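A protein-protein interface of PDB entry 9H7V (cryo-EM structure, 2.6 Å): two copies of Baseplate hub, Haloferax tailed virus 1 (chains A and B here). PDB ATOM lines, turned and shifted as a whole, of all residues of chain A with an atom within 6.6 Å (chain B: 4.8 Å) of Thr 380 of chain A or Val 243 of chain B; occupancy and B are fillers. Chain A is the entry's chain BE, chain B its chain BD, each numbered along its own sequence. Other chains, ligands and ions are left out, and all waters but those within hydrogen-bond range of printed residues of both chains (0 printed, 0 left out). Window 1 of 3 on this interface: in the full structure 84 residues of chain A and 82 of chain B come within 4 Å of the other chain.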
ATOM      1  N   ASN A 376       8.027 -34.654 -18.116  1.00  0.00           N
ATOM      2  CA  ASN A 376       8.394 -34.366 -16.740  1.00  0.00           C
ATOM      3  C   ASN A 376       8.114 -32.886 -16.489  1.00  0.00           C
ATOM      4  O   ASN A 376       7.930 -32.130 -17.441  1.00  0.00           O
ATOM      5  CB  ASN A 376       9.850 -34.750 -16.469  1.00  0.00           C
ATOM      6  CG  ASN A 376      10.165 -36.181 -16.858  1.00  0.00           C
ATOM      7  OD1 ASN A 376       9.846 -37.113 -16.126  1.00  0.00           O
ATOM      8  ND2 ASN A 376      10.787 -36.361 -18.012  1.00  0.00           N
ATOM      9  N   ARG A 377       8.069 -32.476 -15.215  1.00  0.00           N
ATOM     10  CA  ARG A 377       7.688 -31.110 -14.887  1.00  0.00           C
ATOM     11  C   ARG A 377       8.568 -30.546 -13.774  1.00  0.00           C
ATOM     12  O   ARG A 377       8.867 -31.234 -12.801  1.00  0.00           O
ATOM     13  CB  ARG A 377       6.201 -31.038 -14.526  1.00  0.00           C
ATOM     14  CG  ARG A 377       5.710 -29.637 -14.188  1.00  0.00           C
ATOM     15  CD  ARG A 377       4.219 -29.563 -13.955  1.00  0.00           C
ATOM     16  NE  ARG A 377       3.490 -29.068 -15.116  1.00  0.00           N
ATOM     17  CZ  ARG A 377       2.900 -29.820 -16.039  1.00  0.00           C
ATOM     18  NH1 ARG A 377       2.269 -29.244 -17.047  1.00  0.00           N
ATOM     19  NH2 ARG A 377       2.939 -31.140 -15.961  1.00  0.00           N
ATOM     20  N   ILE A 378       8.968 -29.278 -13.943  1.00  0.00           N
ATOM     21  CA  ILE A 378       9.590 -28.493 -12.887  1.00  0.00           C
ATOM     22  C   ILE A 378       8.790 -27.205 -12.676  1.00  0.00           C
ATOM     23  O   ILE A 378       8.462 -26.507 -13.635  1.00  0.00           O
ATOM     24  CB  ILE A 378      11.102 -28.273 -13.137  1.00  0.00           C
ATOM     25  CG1 ILE A 378      11.793 -27.611 -11.939  1.00  0.00           C
ATOM     26  CG2 ILE A 378      11.373 -27.530 -14.440  1.00  0.00           C
ATOM     27  CD1 ILE A 378      13.235 -28.023 -11.745  1.00  0.00           C
ATOM     28  N   THR A 379       8.470 -26.922 -11.406  1.00  0.00           N
ATOM     29  CA  THR A 379       7.633 -25.794 -11.020  1.00  0.00           C
ATOM     30  C   THR A 379       8.508 -24.668 -10.471  1.00  0.00           C
ATOM     31  O   THR A 379       9.339 -24.903  -9.595  1.00  0.00           O
ATOM     32  CB  THR A 379       6.549 -26.220 -10.017  1.00  0.00           C
ATOM     33  OG1 THR A 379       7.179 -26.721  -8.837  1.00  0.00           O
ATOM     34  CG2 THR A 379       5.594 -27.257 -10.569  1.00  0.00           C
ATOM     35  N   THR A 380       8.306 -23.449 -10.991  1.00  0.00           N
ATOM     36  CA  THR A 380       9.079 -22.275 -10.604  1.00  0.00           C
ATOM     37  C   THR A 380       8.279 -21.446  -9.599  1.00  0.00           C
ATOM     38  O   THR A 380       7.183 -20.983  -9.912  1.00  0.00           O
ATOM     39  CB  THR A 380       9.502 -21.460 -11.836  1.00  0.00           C
ATOM     40  OG1 THR A 380      10.185 -22.322 -12.746  1.00  0.00           O
ATOM     41  CG2 THR A 380      10.389 -20.280 -11.501  1.00  0.00           C
ATOM     42  N   THR A 381       8.851 -21.259  -8.402  1.00  0.00           N
ATOM     43  CA  THR A 381       8.174 -20.618  -7.280  1.00  0.00           C
ATOM     44  C   THR A 381       9.106 -19.615  -6.599  1.00  0.00           C
ATOM     45  O   THR A 381      10.290 -19.892  -6.426  1.00  0.00           O
ATOM     46  CB  THR A 381       7.635 -21.661  -6.290  1.00  0.00           C
ATOM     47  OG1 THR A 381       8.648 -22.635  -6.032  1.00  0.00           O
ATOM     48  CG2 THR A 381       6.389 -22.361  -6.784  1.00  0.00           C
ATOM     49  N   ASN A 382       8.548 -18.458  -6.209  1.00  0.00           N
ATOM     50  CA  ASN A 382       9.288 -17.380  -5.564  1.00  0.00           C
ATOM     51  C   ASN A 382       8.680 -17.058  -4.200  1.00  0.00           C
ATOM     52  O   ASN A 382       7.477 -16.833  -4.090  1.00  0.00           O
ATOM     53  CB  ASN A 382       9.261 -16.088  -6.385  1.00  0.00           C
ATOM     54  CG  ASN A 382      10.040 -16.169  -7.679  1.00  0.00           C
ATOM     55  OD1 ASN A 382      11.254 -16.360  -7.673  1.00  0.00           O
ATOM     56  ND2 ASN A 382       9.349 -16.004  -8.795  1.00  0.00           N
ATOM     57  N   HIS A 929       2.968 -21.744  -1.926  1.00  0.00           N
ATOM     58  CA  HIS A 929       2.724 -21.216  -3.261  1.00  0.00           C
ATOM     59  C   HIS A 929       1.508 -21.880  -3.895  1.00  0.00           C
ATOM     60  O   HIS A 929       1.254 -23.059  -3.664  1.00  0.00           O
ATOM     61  CB  HIS A 929       3.921 -21.463  -4.185  1.00  0.00           C
ATOM     62  CG  HIS A 929       5.222 -21.081  -3.577  1.00  0.00           C
ATOM     63  ND1 HIS A 929       5.749 -19.816  -3.707  1.00  0.00           N
ATOM     64  CD2 HIS A 929       6.085 -21.783  -2.815  1.00  0.00           C
ATOM     65  CE1 HIS A 929       6.890 -19.755  -3.056  1.00  0.00           C
ATOM     66  NE2 HIS A 929       7.113 -20.944  -2.497  1.00  0.00           N
ATOM     67  N   LEU A 931       0.105 -23.032  -7.506  1.00  0.00           N
ATOM     68  CA  LEU A 931       0.561 -23.435  -8.825  1.00  0.00           C
ATOM     69  C   LEU A 931      -0.640 -23.466  -9.764  1.00  0.00           C
ATOM     70  O   LEU A 931      -1.766 -23.695  -9.322  1.00  0.00           O
ATOM     71  CB  LEU A 931       1.199 -24.826  -8.719  1.00  0.00           C
ATOM     72  CG  LEU A 931       2.302 -24.990  -7.674  1.00  0.00           C
ATOM     73  CD1 LEU A 931       2.722 -26.447  -7.562  1.00  0.00           C
ATOM     74  CD2 LEU A 931       3.503 -24.119  -8.002  1.00  0.00           C
ATOM     75  N   ALA A 943       9.529 -31.861 -10.114  1.00  0.00           N
ATOM     76  CA  ALA A 943      10.645 -31.217  -9.438  1.00  0.00           C
ATOM     77  C   ALA A 943      10.311 -29.765  -9.094  1.00  0.00           C
ATOM     78  O   ALA A 943       9.414 -29.172  -9.691  1.00  0.00           O
ATOM     79  CB  ALA A 943      11.887 -31.317 -10.289  1.00  0.00           C
ATOM     80  N   SER A 944      11.051 -29.208  -8.124  1.00  0.00           N
ATOM     81  CA  SER A 944      10.874 -27.836  -7.676  1.00  0.00           C
ATOM     82  C   SER A 944      12.009 -26.950  -8.187  1.00  0.00           C
ATOM     83  O   SER A 944      13.138 -27.410  -8.359  1.00  0.00           O
ATOM     84  CB  SER A 944      10.769 -27.768  -6.173  1.00  0.00           C
ATOM     85  OG  SER A 944      12.010 -28.083  -5.559  1.00  0.00           O
ATOM     86  N   SER A 945      11.670 -25.681  -8.436  1.00  0.00           N
ATOM     87  CA  SER A 945      12.618 -24.586  -8.547  1.00  0.00           C
ATOM     88  C   SER A 945      12.162 -23.462  -7.623  1.00  0.00           C
ATOM     89  O   SER A 945      11.557 -22.483  -8.059  1.00  0.00           O
ATOM     90  CB  SER A 945      12.778 -24.129  -9.972  1.00  0.00           C
ATOM     91  OG  SER A 945      13.671 -24.985 -10.663  1.00  0.00           O
ATOM     92  N   GLU A 946      12.453 -23.653  -6.334  1.00  0.00           N
ATOM     93  CA  GLU A 946      11.987 -22.800  -5.256  1.00  0.00           C
ATOM     94  C   GLU A 946      13.062 -21.758  -4.957  1.00  0.00           C
ATOM     95  O   GLU A 946      14.102 -22.084  -4.385  1.00  0.00           O
ATOM     96  CB  GLU A 946      11.677 -23.689  -4.048  1.00  0.00           C
ATOM     97  CG  GLU A 946      11.353 -22.935  -2.771  1.00  0.00           C
ATOM     98  CD  GLU A 946       9.916 -22.474  -2.618  1.00  0.00           C
ATOM     99  OE1 GLU A 946       9.043 -22.980  -3.354  1.00  0.00           O
ATOM    100  OE2 GLU A 946       9.678 -21.613  -1.750  1.00  0.00           O
ATOM    101  N   SER A 947      12.803 -20.510  -5.364  1.00  0.00           N
ATOM    102  CA  SER A 947      13.671 -19.395  -5.029  1.00  0.00           C
ATOM    103  C   SER A 947      13.257 -18.811  -3.682  1.00  0.00           C
ATOM    104  O   SER A 947      12.106 -18.415  -3.503  1.00  0.00           O
ATOM    105  CB  SER A 947      13.654 -18.340  -6.106  1.00  0.00           C
ATOM    106  OG  SER A 947      14.240 -18.827  -7.303  1.00  0.00           O
ATOM    107  N   ASN B 228       5.558 -18.135 -19.988  1.00  0.00           N
ATOM    108  CA  ASN B 228       5.378 -18.738 -18.673  1.00  0.00           C
ATOM    109  C   ASN B 228       5.535 -20.259 -18.703  1.00  0.00           C
ATOM    110  O   ASN B 228       5.495 -20.897 -17.651  1.00  0.00           O
ATOM    111  CB  ASN B 228       4.088 -18.257 -17.999  1.00  0.00           C
ATOM    112  CG  ASN B 228       2.857 -18.366 -18.876  1.00  0.00           C
ATOM    113  OD1 ASN B 228       2.632 -19.382 -19.531  1.00  0.00           O
ATOM    114  ND2 ASN B 228       2.036 -17.329 -18.879  1.00  0.00           N
ATOM    115  N   GLU B 229       5.719 -20.833 -19.898  1.00  0.00           N
ATOM    116  CA  GLU B 229       5.915 -22.267 -20.053  1.00  0.00           C
ATOM    117  C   GLU B 229       6.976 -22.511 -21.122  1.00  0.00           C
ATOM    118  O   GLU B 229       6.897 -21.955 -22.215  1.00  0.00           O
ATOM    119  CB  GLU B 229       4.589 -22.955 -20.389  1.00  0.00           C
ATOM    120  CG  GLU B 229       4.658 -24.474 -20.383  1.00  0.00           C
ATOM    121  CD  GLU B 229       3.313 -25.181 -20.389  1.00  0.00           C
ATOM    122  OE1 GLU B 229       2.531 -24.976 -19.440  1.00  0.00           O
ATOM    123  OE2 GLU B 229       3.048 -25.937 -21.340  1.00  0.00           O
ATOM    124  N   VAL B 230       7.980 -23.327 -20.780  1.00  0.00           N
ATOM    125  CA  VAL B 230       8.962 -23.799 -21.745  1.00  0.00           C
ATOM    126  C   VAL B 230       8.991 -25.323 -21.683  1.00  0.00           C
ATOM    127  O   VAL B 230       9.149 -25.897 -20.608  1.00  0.00           O
ATOM    128  CB  VAL B 230      10.361 -23.188 -21.515  1.00  0.00           C
ATOM    129  CG1 VAL B 230      11.437 -23.885 -22.333  1.00  0.00           C
ATOM    130  CG2 VAL B 230      10.389 -21.698 -21.809  1.00  0.00           C
ATOM    131  N   VAL B 241      10.814 -32.197 -20.766  1.00  0.00           N
ATOM    132  CA  VAL B 241      10.565 -31.554 -19.482  1.00  0.00           C
ATOM    133  C   VAL B 241       9.875 -30.205 -19.701  1.00  0.00           C
ATOM    134  O   VAL B 241      10.247 -29.443 -20.591  1.00  0.00           O
ATOM    135  CB  VAL B 241      11.828 -31.463 -18.595  1.00  0.00           C
ATOM    136  CG1 VAL B 241      12.916 -30.568 -19.172  1.00  0.00           C
ATOM    137  CG2 VAL B 241      11.509 -31.077 -17.157  1.00  0.00           C
ATOM    138  N   ILE B 242       8.854 -29.946 -18.872  1.00  0.00           N
ATOM    139  CA  ILE B 242       8.083 -28.713 -18.867  1.00  0.00           C
ATOM    140  C   ILE B 242       8.558 -27.853 -17.696  1.00  0.00           C
ATOM    141  O   ILE B 242       8.590 -28.316 -16.557  1.00  0.00           O
ATOM    142  CB  ILE B 242       6.568 -29.015 -18.783  1.00  0.00           C
ATOM    143  CG1 ILE B 242       6.093 -29.927 -19.920  1.00  0.00           C
ATOM    144  CG2 ILE B 242       5.756 -27.727 -18.724  1.00  0.00           C
ATOM    145  CD1 ILE B 242       4.753 -30.592 -19.680  1.00  0.00           C
ATOM    146  N   VAL B 243       8.927 -26.601 -17.999  1.00  0.00           N
ATOM    147  CA  VAL B 243       9.267 -25.602 -16.998  1.00  0.00           C
ATOM    148  C   VAL B 243       8.073 -24.660 -16.859  1.00  0.00           C
ATOM    149  O   VAL B 243       7.637 -24.057 -17.838  1.00  0.00           O
ATOM    150  CB  VAL B 243      10.571 -24.851 -17.342  1.00  0.00           C
ATOM    151  CG1 VAL B 243      11.048 -23.991 -16.182  1.00  0.00           C
ATOM    152  CG2 VAL B 243      11.682 -25.794 -17.780  1.00  0.00           C
ATOM    153  N   ASP B 244       7.574 -24.535 -15.624  1.00  0.00           N
ATOM    154  CA  ASP B 244       6.222 -24.070 -15.351  1.00  0.00           C
ATOM    155  C   ASP B 244       6.276 -22.864 -14.412  1.00  0.00           C
ATOM    156  O   ASP B 244       6.612 -23.011 -13.237  1.00  0.00           O
ATOM    157  CB  ASP B 244       5.406 -25.229 -14.765  1.00  0.00           C
ATOM    158  CG  ASP B 244       3.907 -25.178 -15.013  1.00  0.00           C
ATOM    159  OD1 ASP B 244       3.361 -24.062 -15.138  1.00  0.00           O
ATOM    160  OD2 ASP B 244       3.291 -26.262 -15.068  1.00  0.00           O
ATOM    161  N   ASP B 245       5.951 -21.675 -14.944  1.00  0.00           N
ATOM    162  CA  ASP B 245       5.871 -20.449 -14.160  1.00  0.00           C
ATOM    163  C   ASP B 245       4.411 -20.189 -13.796  1.00  0.00           C
ATOM    164  O   ASP B 245       3.716 -19.443 -14.485  1.00  0.00           O
ATOM    165  CB  ASP B 245       6.551 -19.273 -14.875  1.00  0.00           C
ATOM    166  CG  ASP B 245       6.615 -17.970 -14.087  1.00  0.00           C
ATOM    167  OD1 ASP B 245       6.274 -17.974 -12.883  1.00  0.00           O
ATOM    168  OD2 ASP B 245       7.018 -16.954 -14.686  1.00  0.00           O
ATOM    169  N   GLY B 246       3.972 -20.813 -12.694  1.00  0.00           N
ATOM    170  CA  GLY B 246       2.581 -20.836 -12.268  1.00  0.00           C
ATOM    171  C   GLY B 246       2.018 -19.452 -11.951  1.00  0.00           C
ATOM    172  O   GLY B 246       0.844 -19.195 -12.207  1.00  0.00           O
ATOM    173  N   GLU B 280      16.284 -28.991 -17.722  1.00  0.00           N
ATOM    174  CA  GLU B 280      15.561 -28.111 -16.815  1.00  0.00           C
ATOM    175  C   GLU B 280      16.204 -26.727 -16.808  1.00  0.00           C
ATOM    176  O   GLU B 280      15.499 -25.727 -16.927  1.00  0.00           O
ATOM    177  CB  GLU B 280      15.559 -28.674 -15.393  1.00  0.00           C
ATOM    178  CG  GLU B 280      14.532 -29.766 -15.156  1.00  0.00           C
ATOM    179  CD  GLU B 280      14.661 -30.494 -13.827  1.00  0.00           C
ATOM    180  OE1 GLU B 280      15.561 -30.146 -13.032  1.00  0.00           O
ATOM    181  OE2 GLU B 280      13.855 -31.412 -13.586  1.00  0.00           O
ATOM    182  N   GLY B 283      15.677 -24.637 -19.903  1.00  0.00           N
ATOM    183  CA  GLY B 283      14.333 -24.083 -19.868  1.00  0.00           C
ATOM    184  C   GLY B 283      14.212 -22.915 -18.894  1.00  0.00           C
ATOM    185  O   GLY B 283      13.540 -21.929 -19.195  1.00  0.00           O
ATOM    186  N   ARG B 284      14.873 -23.043 -17.735  1.00  0.00           N
ATOM    187  CA  ARG B 284      14.861 -22.018 -16.704  1.00  0.00           C
ATOM    188  C   ARG B 284      15.614 -20.779 -17.181  1.00  0.00           C
ATOM    189  O   ARG B 284      15.178 -19.664 -16.906  1.00  0.00           O
ATOM    190  CB  ARG B 284      15.436 -22.543 -15.387  1.00  0.00           C
ATOM    191  CG  ARG B 284      14.531 -23.522 -14.652  1.00  0.00           C
ATOM    192  CD  ARG B 284      14.929 -23.730 -13.204  1.00  0.00           C
ATOM    193  NE  ARG B 284      16.367 -23.739 -12.961  1.00  0.00           N
ATOM    194  CZ  ARG B 284      17.048 -22.773 -12.349  1.00  0.00           C
ATOM    195  NH1 ARG B 284      18.354 -22.888 -12.191  1.00  0.00           N
ATOM    196  NH2 ARG B 284      16.425 -21.700 -11.892  1.00  0.00           N
ATOM    197  N   LEU B 287      13.404 -18.835 -19.701  1.00  0.00           N
ATOM    198  CA  LEU B 287      12.404 -18.052 -18.986  1.00  0.00           C
ATOM    199  C   LEU B 287      13.049 -16.836 -18.320  1.00  0.00           C
ATOM    200  O   LEU B 287      12.500 -15.738 -18.391  1.00  0.00           O
ATOM    201  CB  LEU B 287      11.706 -18.924 -17.936  1.00  0.00           C
ATOM    202  CG  LEU B 287      10.646 -19.907 -18.437  1.00  0.00           C
ATOM    203  CD1 LEU B 287      10.033 -20.661 -17.269  1.00  0.00           C
ATOM    204  CD2 LEU B 287       9.551 -19.199 -19.221  1.00  0.00           C
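The backbone NH (N) of Ile 242 of chain B sits at hydrogen-bond distance from the backbone carbonyl oxygen (O) of Asn 376 of chain A (2.8 Å). The backbone carbonyl oxygen of Ile 242 of chain B is in hydrogen-bond range of the backbone NH of Ile 378 of chain A (2.8 Å). OD2 of Asp 244 of chain B is in salt-bridge range of NE of Arg 377 of chain A (2.8 Å). N of Asp 244 of chain B is in hydrogen-bond range of O of Ile 378 of chain A (2.9 Å). The backbone carbonyl oxygen (O) of Asp 244 of chain B is in hydrogen-bond range of the backbone NH (N) of Thr 380 of chain A.
The backbone carbonyl oxygen of Val 230 of chain B sits at hydrogen-bond distance from the backbone NH of Val 243 of chain B (2.7 Å). O of Arg 377 of chain A is in hydrogen-bond range of N of Ala 943 of chain A, 2.8 Å away. N of Thr 379 of chain A is in hydrogen-bond range of O of Ala 943 of chain A. The backbone NH (N) of Ser 945 of chain A sits at hydrogen-bond distance from the backbone carbonyl oxygen (O) of Thr 379 of chain A, 2.7 Å away. The backbone NH of Thr 381 of chain A sits at hydrogen-bond distance from the backbone carbonyl oxygen of Ser 945 of chain A (3.0 Å).
O of Asn 376 of chain A touches CA of Val 241 of chain B, 3.4 Å away. Ile 242 of chain B touches Arg 377 of chain A. Ile 378 of chain A touches Val 243 of chain B. Ile 378 of chain A touches Glu 280 of chain B (CD1 to OE1, 3.4 Å). Thr 379 of chain A touches Asp 244 of chain B. OG1 of Thr 380 of chain A touches CG1 of Val 243 of chain B, at 3.9 Å. Ala 943 of chain A touches Glu 280 of chain B. Ser 945 of chain A touches Arg 284 of chain B.
Of the printed residues of chain B, Asn 376 of chain A touches Val 241 and Ile 242. Printed residues of chain B within 4 Å of Arg 377 of chain A: Ile 242 (3.4 Å) and Asp 244 (2.8 Å). Of the printed residues of chain B, Ile 378 of chain A touches Ile 242 (2.8 Å), Val 243 (3.6 Å), Asp 244 (2.9 Å) and Glu 280 (3.4 Å). Thr 380 of chain A touches two residues of chain B. Thr 381 of chain A touches none of the printed residues of chain B. Printed residues of chain B within 4 Å of Ser 945 of chain A: Arg 284. Of the printed residues of chain A, Val 241 of chain B touches Asn 376. Of chain A, only Ile 378 (3.6 Å) and Thr 380 (3.9 Å) come within 4 Å of Val 243 of chain B. The nearest residue of chain B that does not touch Thr 380 of chain A is Gly 246 of chain B (4.3 Å). The nearest printed residue of chain A that does not touch Val 243 of chain B is Arg 377 of chain A (5.6 Å).
Hydrophobic or aromatic side chains of chain A that line the printed part of chain B: Ile 378 and Ala 943. Of the 13 printed residues of chain B, 6 touch a printed residue of chain A. Printed residues of chain B that touch a printed residue of chain A: Val 241, Ile 242, Val 243, Asp 244, Glu 280 and Arg 284.
No position is printed for both chains. Of the 13 pairs that touch across the chains among the printed residues, none has its exchanged pair printed and touching as well.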
